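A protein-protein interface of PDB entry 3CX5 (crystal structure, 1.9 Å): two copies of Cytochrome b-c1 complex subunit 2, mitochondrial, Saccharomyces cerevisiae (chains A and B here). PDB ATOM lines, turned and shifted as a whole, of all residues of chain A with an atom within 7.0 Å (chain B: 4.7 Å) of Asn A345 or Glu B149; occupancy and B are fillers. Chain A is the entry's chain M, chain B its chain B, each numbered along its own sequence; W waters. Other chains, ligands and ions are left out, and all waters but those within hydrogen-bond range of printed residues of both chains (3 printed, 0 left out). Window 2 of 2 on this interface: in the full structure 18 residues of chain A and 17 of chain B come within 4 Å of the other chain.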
ATOM      1  N   ARG A 214      20.129  11.322  30.748  1.00  0.00           N
ATOM      2  CA  ARG A 214      19.382  10.196  30.193  1.00  0.00           C
ATOM      3  C   ARG A 214      20.145   9.523  29.049  1.00  0.00           C
ATOM      4  O   ARG A 214      20.690  10.197  28.168  1.00  0.00           O
ATOM      5  CB  ARG A 214      18.005  10.688  29.728  1.00  0.00           C
ATOM      6  CG  ARG A 214      17.290  11.560  30.784  1.00  0.00           C
ATOM      7  CD  ARG A 214      15.951  12.104  30.300  1.00  0.00           C
ATOM      8  NE  ARG A 214      14.917  11.075  30.248  1.00  0.00           N
ATOM      9  CZ  ARG A 214      14.347  10.525  31.317  1.00  0.00           C
ATOM     10  NH1 ARG A 214      13.417   9.593  31.166  1.00  0.00           N
ATOM     11  NH2 ARG A 214      14.696  10.912  32.538  1.00  0.00           N
ATOM     12  N   ARG A 216      19.842   6.425  26.093  1.00  0.00           N
ATOM     13  CA  ARG A 216      19.061   5.420  25.381  1.00  0.00           C
ATOM     14  C   ARG A 216      19.897   4.141  25.336  1.00  0.00           C
ATOM     15  O   ARG A 216      21.106   4.192  25.104  1.00  0.00           O
ATOM     16  CB  ARG A 216      18.738   5.881  23.963  1.00  0.00           C
ATOM     17  CG  ARG A 216      18.145   7.277  23.887  1.00  0.00           C
ATOM     18  CD  ARG A 216      17.437   7.480  22.567  1.00  0.00           C
ATOM     19  NE  ARG A 216      16.245   6.645  22.481  1.00  0.00           N
ATOM     20  CZ  ARG A 216      15.460   6.569  21.414  1.00  0.00           C
ATOM     21  NH1 ARG A 216      14.392   5.784  21.427  1.00  0.00           N
ATOM     22  NH2 ARG A 216      15.763   7.258  20.320  1.00  0.00           N
ATOM     23  N   PHE A 217      19.249   3.000  25.552  1.00  0.00           N
ATOM     24  CA  PHE A 217      19.939   1.715  25.566  1.00  0.00           C
ATOM     25  C   PHE A 217      18.958   0.580  25.292  1.00  0.00           C
ATOM     26  O   PHE A 217      17.817   0.606  25.762  1.00  0.00           O
ATOM     27  CB  PHE A 217      20.615   1.527  26.933  1.00  0.00           C
ATOM     28  CG  PHE A 217      21.154   0.142  27.181  1.00  0.00           C
ATOM     29  CD1 PHE A 217      22.403  -0.235  26.692  1.00  0.00           C
ATOM     30  CD2 PHE A 217      20.428  -0.773  27.948  1.00  0.00           C
ATOM     31  CE1 PHE A 217      22.926  -1.502  26.964  1.00  0.00           C
ATOM     32  CE2 PHE A 217      20.942  -2.041  28.226  1.00  0.00           C
ATOM     33  CZ  PHE A 217      22.195  -2.407  27.735  1.00  0.00           C
ATOM     34  N   ILE A 218      19.393  -0.386  24.485  1.00  0.00           N
ATOM     35  CA  ILE A 218      18.563  -1.537  24.154  1.00  0.00           C
ATOM     36  C   ILE A 218      18.820  -2.636  25.176  1.00  0.00           C
ATOM     37  O   ILE A 218      19.936  -3.152  25.286  1.00  0.00           O
ATOM     38  CB  ILE A 218      18.874  -2.096  22.747  1.00  0.00           C
ATOM     39  CG1 ILE A 218      18.682  -1.006  21.687  1.00  0.00           C
ATOM     40  CG2 ILE A 218      17.969  -3.296  22.447  1.00  0.00           C
ATOM     41  CD1 ILE A 218      18.921  -1.485  20.272  1.00  0.00           C
ATOM     42  N   SER A 221      15.850  -1.641  31.429  1.00  0.00           N
ATOM     43  CA  SER A 221      15.811  -0.225  31.788  1.00  0.00           C
ATOM     44  C   SER A 221      16.264  -0.066  33.236  1.00  0.00           C
ATOM     45  O   SER A 221      16.087  -0.964  34.063  1.00  0.00           O
ATOM     46  CB  SER A 221      14.409   0.360  31.622  1.00  0.00           C
ATOM     47  OG  SER A 221      14.147   0.711  30.274  1.00  0.00           O
ATOM     48  N   ASP A 277      10.951  -4.302  32.040  1.00  0.00           N
ATOM     49  CA  ASP A 277       9.749  -3.511  31.786  1.00  0.00           C
ATOM     50  C   ASP A 277       9.954  -2.091  32.322  1.00  0.00           C
ATOM     51  O   ASP A 277      10.229  -1.899  33.506  1.00  0.00           O
ATOM     52  CB  ASP A 277       8.552  -4.182  32.475  1.00  0.00           C
ATOM     53  CG  ASP A 277       7.209  -3.586  32.071  1.00  0.00           C
ATOM     54  OD1 ASP A 277       6.184  -4.218  32.401  1.00  0.00           O
ATOM     55  OD2 ASP A 277       7.156  -2.504  31.439  1.00  0.00           O
ATOM     56  N   SER A 278       9.814  -1.102  31.446  1.00  0.00           N
ATOM     57  CA  SER A 278       9.995   0.290  31.840  1.00  0.00           C
ATOM     58  C   SER A 278       8.923   0.757  32.831  1.00  0.00           C
ATOM     59  O   SER A 278       9.201   1.577  33.706  1.00  0.00           O
ATOM     60  CB  SER A 278      10.028   1.197  30.607  1.00  0.00           C
ATOM     61  OG  SER A 278       8.898   0.972  29.782  1.00  0.00           O
ATOM     62  N   ALA A 279       7.720   0.195  32.722  1.00  0.00           N
ATOM     63  CA  ALA A 279       6.619   0.554  33.616  1.00  0.00           C
ATOM     64  C   ALA A 279       6.930   0.139  35.050  1.00  0.00           C
ATOM     65  O   ALA A 279       6.624   0.869  35.996  1.00  0.00           O
ATOM     66  CB  ALA A 279       5.318  -0.092  33.148  1.00  0.00           C
ATOM     67  N   VAL A 281       9.960  -0.246  36.314  1.00  0.00           N
ATOM     68  CA  VAL A 281      11.050   0.591  36.807  1.00  0.00           C
ATOM     69  C   VAL A 281      10.478   1.936  37.275  1.00  0.00           C
ATOM     70  O   VAL A 281      10.834   2.424  38.341  1.00  0.00           O
ATOM     71  CB  VAL A 281      12.125   0.837  35.726  1.00  0.00           C
ATOM     72  CG1 VAL A 281      13.262   1.676  36.293  1.00  0.00           C
ATOM     73  CG2 VAL A 281      12.665  -0.490  35.205  1.00  0.00           C
ATOM     74  N   SER A 282       9.566   2.493  36.479  1.00  0.00           N
ATOM     75  CA  SER A 282       8.916   3.766  36.781  1.00  0.00           C
ATOM     76  C   SER A 282       8.141   3.736  38.092  1.00  0.00           C
ATOM     77  O   SER A 282       8.288   4.634  38.924  1.00  0.00           O
ATOM     78  CB  SER A 282       7.974   4.165  35.647  1.00  0.00           C
ATOM     79  OG  SER A 282       8.698   4.389  34.451  1.00  0.00           O
ATOM     80  N   GLY A 341      17.997   3.197  29.198  1.00  0.00           N
ATOM     81  CA  GLY A 341      17.155   2.214  28.549  1.00  0.00           C
ATOM     82  C   GLY A 341      16.031   2.841  27.762  1.00  0.00           C
ATOM     83  O   GLY A 341      16.272   3.662  26.870  1.00  0.00           O
ATOM     84  N   ASP A 342      14.804   2.429  28.082  1.00  0.00           N
ATOM     85  CA  ASP A 342      13.586   2.927  27.442  1.00  0.00           C
ATOM     86  C   ASP A 342      13.256   4.291  28.073  1.00  0.00           C
ATOM     87  O   ASP A 342      12.210   4.477  28.707  1.00  0.00           O
ATOM     88  CB  ASP A 342      12.446   1.924  27.670  1.00  0.00           C
ATOM     89  CG  ASP A 342      11.204   2.231  26.840  1.00  0.00           C
ATOM     90  OD1 ASP A 342      10.150   1.607  27.098  1.00  0.00           O
ATOM     91  OD2 ASP A 342      11.273   3.087  25.931  1.00  0.00           O
ATOM     92  N   VAL A 343      14.173   5.231  27.867  1.00  0.00           N
ATOM     93  CA  VAL A 343      14.108   6.590  28.388  1.00  0.00           C
ATOM     94  C   VAL A 343      12.813   7.365  28.132  1.00  0.00           C
ATOM     95  O   VAL A 343      12.395   8.154  28.982  1.00  0.00           O
ATOM     96  CB  VAL A 343      15.360   7.390  27.918  1.00  0.00           C
ATOM     97  CG1 VAL A 343      15.145   8.882  28.039  1.00  0.00           C
ATOM     98  CG2 VAL A 343      16.568   6.977  28.757  1.00  0.00           C
ATOM     99  N   SER A 344      12.171   7.132  26.988  1.00  0.00           N
ATOM    100  CA  SER A 344      10.921   7.817  26.665  1.00  0.00           C
ATOM    101  C   SER A 344       9.768   7.383  27.569  1.00  0.00           C
ATOM    102  O   SER A 344       8.716   8.031  27.613  1.00  0.00           O
ATOM    103  CB  SER A 344      10.543   7.578  25.203  1.00  0.00           C
ATOM    104  OG  SER A 344      11.467   8.213  24.335  1.00  0.00           O
ATOM    105  N   ASN A 345       9.974   6.290  28.296  1.00  0.00           N
ATOM    106  CA  ASN A 345       8.956   5.760  29.194  1.00  0.00           C
ATOM    107  C   ASN A 345       9.493   5.596  30.610  1.00  0.00           C
ATOM    108  O   ASN A 345       9.031   4.742  31.367  1.00  0.00           O
ATOM    109  CB  ASN A 345       8.421   4.431  28.653  1.00  0.00           C
ATOM    110  CG  ASN A 345       7.725   4.590  27.316  1.00  0.00           C
ATOM    111  OD1 ASN A 345       6.631   5.148  27.238  1.00  0.00           O
ATOM    112  ND2 ASN A 345       8.375   4.139  26.250  1.00  0.00           N
ATOM    113  N   LEU A 346      10.482   6.417  30.951  1.00  0.00           N
ATOM    114  CA  LEU A 346      11.099   6.406  32.274  1.00  0.00           C
ATOM    115  C   LEU A 346      10.835   7.772  32.923  1.00  0.00           C
ATOM    116  O   LEU A 346      10.671   8.775  32.224  1.00  0.00           O
ATOM    117  CB  LEU A 346      12.602   6.139  32.150  1.00  0.00           C
ATOM    118  CG  LEU A 346      13.159   4.781  32.607  1.00  0.00           C
ATOM    119  CD1 LEU A 346      12.095   3.704  32.600  1.00  0.00           C
ATOM    120  CD2 LEU A 346      14.356   4.382  31.744  1.00  0.00           C
ATOM    121  N   PRO A 347      10.787   7.829  34.265  1.00  0.00           N
ATOM    122  CA  PRO A 347      10.528   9.117  34.923  1.00  0.00           C
ATOM    123  C   PRO A 347      11.659  10.130  34.796  1.00  0.00           C
ATOM    124  O   PRO A 347      12.823   9.772  34.620  1.00  0.00           O
ATOM    125  CB  PRO A 347      10.321   8.725  36.392  1.00  0.00           C
ATOM    126  CG  PRO A 347       9.928   7.267  36.330  1.00  0.00           C
ATOM    127  CD  PRO A 347      10.854   6.746  35.258  1.00  0.00           C
ATOM    128  N   TYR A 348      11.287  11.402  34.855  1.00  0.00           N
ATOM    129  CA  TYR A 348      12.243  12.498  34.803  1.00  0.00           C
ATOM    130  C   TYR A 348      12.419  12.984  36.239  1.00  0.00           C
ATOM    131  O   TYR A 348      11.541  12.764  37.079  1.00  0.00           O
ATOM    132  CB  TYR A 348      11.703  13.638  33.940  1.00  0.00           C
ATOM    133  CG  TYR A 348      11.623  13.312  32.472  1.00  0.00           C
ATOM    134  CD1 TYR A 348      12.609  13.757  31.587  1.00  0.00           C
ATOM    135  CD2 TYR A 348      10.562  12.564  31.960  1.00  0.00           C
ATOM    136  CE1 TYR A 348      12.540  13.465  30.224  1.00  0.00           C
ATOM    137  CE2 TYR A 348      10.482  12.268  30.599  1.00  0.00           C
ATOM    138  CZ  TYR A 348      11.476  12.722  29.737  1.00  0.00           C
ATOM    139  OH  TYR A 348      11.400  12.445  28.388  1.00  0.00           O
ATOM    140  N   LYS B  28       4.830   5.271  19.565  1.00  0.00           N
ATOM    141  CA  LYS B  28       5.969   4.560  20.145  1.00  0.00           C
ATOM    142  C   LYS B  28       7.192   5.042  19.371  1.00  0.00           C
ATOM    143  O   LYS B  28       7.069   5.449  18.216  1.00  0.00           O
ATOM    144  CB  LYS B  28       5.799   3.043  19.993  1.00  0.00           C
ATOM    145  CG  LYS B  28       4.470   2.520  20.524  1.00  0.00           C
ATOM    146  CD  LYS B  28       4.363   1.004  20.459  1.00  0.00           C
ATOM    147  CE  LYS B  28       5.277   0.339  21.471  1.00  0.00           C
ATOM    148  NZ  LYS B  28       5.055  -1.135  21.541  1.00  0.00           N
ATOM    149  N   ASP B  29       8.356   5.027  20.016  1.00  0.00           N
ATOM    150  CA  ASP B  29       9.591   5.482  19.382  1.00  0.00           C
ATOM    151  C   ASP B  29       9.916   4.806  18.051  1.00  0.00           C
ATOM    152  O   ASP B  29      10.079   3.586  17.980  1.00  0.00           O
ATOM    153  CB  ASP B  29      10.771   5.338  20.349  1.00  0.00           C
ATOM    154  CG  ASP B  29      10.723   6.346  21.489  1.00  0.00           C
ATOM    155  OD1 ASP B  29       9.766   7.152  21.555  1.00  0.00           O
ATOM    156  OD2 ASP B  29      11.652   6.341  22.320  1.00  0.00           O
ATOM    157  N   LYS B 137       8.143  14.172  25.769  1.00  0.00           N
ATOM    158  CA  LYS B 137       7.137  13.337  25.095  1.00  0.00           C
ATOM    159  C   LYS B 137       6.487  13.772  23.768  1.00  0.00           C
ATOM    160  O   LYS B 137       6.237  12.932  22.910  1.00  0.00           O
ATOM    161  CB  LYS B 137       6.043  12.932  26.081  1.00  0.00           C
ATOM    162  CG  LYS B 137       5.283  11.681  25.671  1.00  0.00           C
ATOM    163  CD  LYS B 137       6.182  10.459  25.749  1.00  0.00           C
ATOM    164  CE  LYS B 137       5.403   9.181  25.507  1.00  0.00           C
ATOM    165  NZ  LYS B 137       6.215   7.995  25.880  1.00  0.00           N
ATOM    166  N   TYR B 145      13.783   5.191  14.121  1.00  0.00           N
ATOM    167  CA  TYR B 145      13.641   3.964  14.899  1.00  0.00           C
ATOM    168  C   TYR B 145      15.019   3.402  15.218  1.00  0.00           C
ATOM    169  O   TYR B 145      15.829   3.172  14.310  1.00  0.00           O
ATOM    170  CB  TYR B 145      12.834   2.932  14.103  1.00  0.00           C
ATOM    171  CG  TYR B 145      12.686   1.585  14.781  1.00  0.00           C
ATOM    172  CD1 TYR B 145      13.302   0.444  14.254  1.00  0.00           C
ATOM    173  CD2 TYR B 145      11.918   1.446  15.938  1.00  0.00           C
ATOM    174  CE1 TYR B 145      13.150  -0.802  14.866  1.00  0.00           C
ATOM    175  CE2 TYR B 145      11.760   0.206  16.554  1.00  0.00           C
ATOM    176  CZ  TYR B 145      12.377  -0.912  16.013  1.00  0.00           C
ATOM    177  OH  TYR B 145      12.218  -2.134  16.626  1.00  0.00           O
ATOM    178  N   GLY B 147      15.202   0.888  17.885  1.00  0.00           N
ATOM    179  CA  GLY B 147      14.959  -0.354  18.594  1.00  0.00           C
ATOM    180  C   GLY B 147      14.925  -0.362  20.113  1.00  0.00           C
ATOM    181  O   GLY B 147      14.782  -1.436  20.693  1.00  0.00           O
ATOM    182  N   VAL B 148      15.062   0.789  20.773  1.00  0.00           N
ATOM    183  CA  VAL B 148      15.016   0.791  22.239  1.00  0.00           C
ATOM    184  C   VAL B 148      13.601   0.419  22.689  1.00  0.00           C
ATOM    185  O   VAL B 148      13.416  -0.264  23.702  1.00  0.00           O
ATOM    186  CB  VAL B 148      15.448   2.147  22.870  1.00  0.00           C
ATOM    187  CG1 VAL B 148      16.814   2.574  22.345  1.00  0.00           C
ATOM    188  CG2 VAL B 148      14.407   3.209  22.624  1.00  0.00           C
ATOM    189  N   GLU B 149      12.613   0.852  21.908  1.00  0.00           N
ATOM    190  CA  GLU B 149      11.216   0.539  22.177  1.00  0.00           C
ATOM    191  C   GLU B 149      10.737  -0.344  21.027  1.00  0.00           C
ATOM    192  O   GLU B 149      10.642   0.103  19.884  1.00  0.00           O
ATOM    193  CB  GLU B 149      10.370   1.817  22.278  1.00  0.00           C
ATOM    194  CG  GLU B 149       8.894   1.556  22.578  1.00  0.00           C
ATOM    195  CD  GLU B 149       8.118   2.798  23.018  1.00  0.00           C
ATOM    196  OE1 GLU B 149       8.602   3.935  22.806  1.00  0.00           O
ATOM    197  OE2 GLU B 149       7.010   2.626  23.580  1.00  0.00           O
ATOM    198  N   ARG B 150      10.486  -1.611  21.342  1.00  0.00           N
ATOM    199  CA  ARG B 150      10.038  -2.613  20.374  1.00  0.00           C
ATOM    200  C   ARG B 150       8.769  -2.168  19.639  1.00  0.00           C
ATOM    201  O   ARG B 150       7.776  -1.812  20.269  1.00  0.00           O
ATOM    202  CB  ARG B 150       9.788  -3.930  21.117  1.00  0.00           C
ATOM    203  CG  ARG B 150       9.826  -5.206  20.279  1.00  0.00           C
ATOM    204  CD  ARG B 150       9.635  -6.415  21.204  1.00  0.00           C
ATOM    205  NE  ARG B 150       9.736  -7.706  20.523  1.00  0.00           N
ATOM    206  CZ  ARG B 150       9.372  -8.870  21.062  1.00  0.00           C
ATOM    207  NH1 ARG B 150       9.503  -9.994  20.369  1.00  0.00           N
ATOM    208  NH2 ARG B 150       8.868  -8.915  22.292  1.00  0.00           N
ATOM    209  N   VAL B 151       8.824  -2.165  18.308  1.00  0.00           N
ATOM    210  CA  VAL B 151       7.687  -1.767  17.475  1.00  0.00           C
ATOM    211  C   VAL B 151       7.265  -2.912  16.550  1.00  0.00           C
ATOM    212  O   VAL B 151       8.012  -3.316  15.653  1.00  0.00           O
ATOM    213  CB  VAL B 151       8.018  -0.517  16.626  1.00  0.00           C
ATOM    214  CG1 VAL B 151       6.838  -0.163  15.713  1.00  0.00           C
ATOM    215  CG2 VAL B 151       8.366   0.662  17.530  1.00  0.00           C
HETATM  216  O   HOH W   1      12.639   4.991  24.747  1.00  0.00           O
HETATM  217  O   HOH W   2      15.187  -0.845  26.502  1.00  0.00           O
HETATM  218  O   HOH W   3       9.047   9.772  23.150  1.00  0.00           O
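The side-chain amide oxygen (OD1) of Asn A345 is in hydrogen-bond range of the side-chain amino group (NZ) of Lys B137 (3.2 Å).
O of Ser A344 sits at hydrogen-bond distance from NZ of Lys B137, at 3.0 Å.
The side-chain carboxylate (OD2) of Asp B29 sits at hydrogen-bond distance from the side-chain hydroxyl (OG) of Ser A344 (2.8 Å).
NH1 of Arg A216 lies within salt-bridge range of OD2 of Asp B29 (2.9 Å).
The side-chain carboxylate (OE2) of Glu B149 lies within hydrogen-bond range of the side-chain amide nitrogen (ND2) of Asn A345, 3.4 Å away.
The side-chain hydroxyl (OG) of Ser A221 is in hydrogen-bond range of the backbone NH (N) of Asp A342, at 2.9 Å.
The side-chain carboxylate (OD2) of Asp A342 is in hydrogen-bond range of the side-chain amide nitrogen (ND2) of Asn A345 (3.1 Å).
The backbone carbonyl oxygen (O) of Asn A345 lies within hydrogen-bond range of the side-chain hydroxyl (OG) of Ser A282 (3.1 Å).
The side-chain carboxylate of Asp A342 sits at hydrogen-bond distance from the side-chain hydroxyl of Ser A278, 3.0 Å away.
The backbone NH (N) of Asp B29 lies within hydrogen-bond range of the side-chain carboxylate (OE1) of Glu B149 (3.0 Å).
Among the printed residues, merely in contact across the chains: Arg A216 with Val B148 (2.8 Å) and Asp A342 with Glu B149 (3.97 Å).
Of the printed residues of chain B, Asp A342 touches Glu B149.
Printed residues of chain B within 4 Å of Ser A344: Asp B29 (2.8 Å) and Lys B137 (3.0 Å).
Of the printed residues of chain B, Asn A345 touches Lys B137 and Glu B149.
Printed residues of chain A within 4 Å of Asp B29: Arg A216 and Ser A344.
Printed residues of chain A within 4 Å of Lys B137: Ser A344 and Asn A345.
Printed residues of chain A within 4 Å of Val B148: Arg A216 (2.8 Å).
Glu B149 touches just these residues of chain A: Asp A342 and Asn A345.
The nearest residue of chain A that does not touch Glu B149 is Ser A344 (4.8 Å).
Hydrophobic or aromatic side chains of chain B that line the printed part of chain A: Val B148.
Along chain B the printed residues that touch a printed residue of chain A span positions 29 to 149.
No position is printed for both chains.
Of the 7 pairs that touch across the chains among the printed residues, none has its exchanged pair printed and touching as well.
Water W1 lies within hydrogen-bond range of OD2 of Asp A342 (2.6 Å), OD2 of Asp B29 (2.9 Å), N of Ser A344 (3.1 Å) and N of Val A343 (3.5 Å).
Water W2 lies within hydrogen-bond range of O of Phe A217 (3.1 Å) and O of Val B148 (3.4 Å).
Water W3 bridges OG of Ser A344 (3.1 Å) and OD1 of Asp B29 (3.2 Å).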
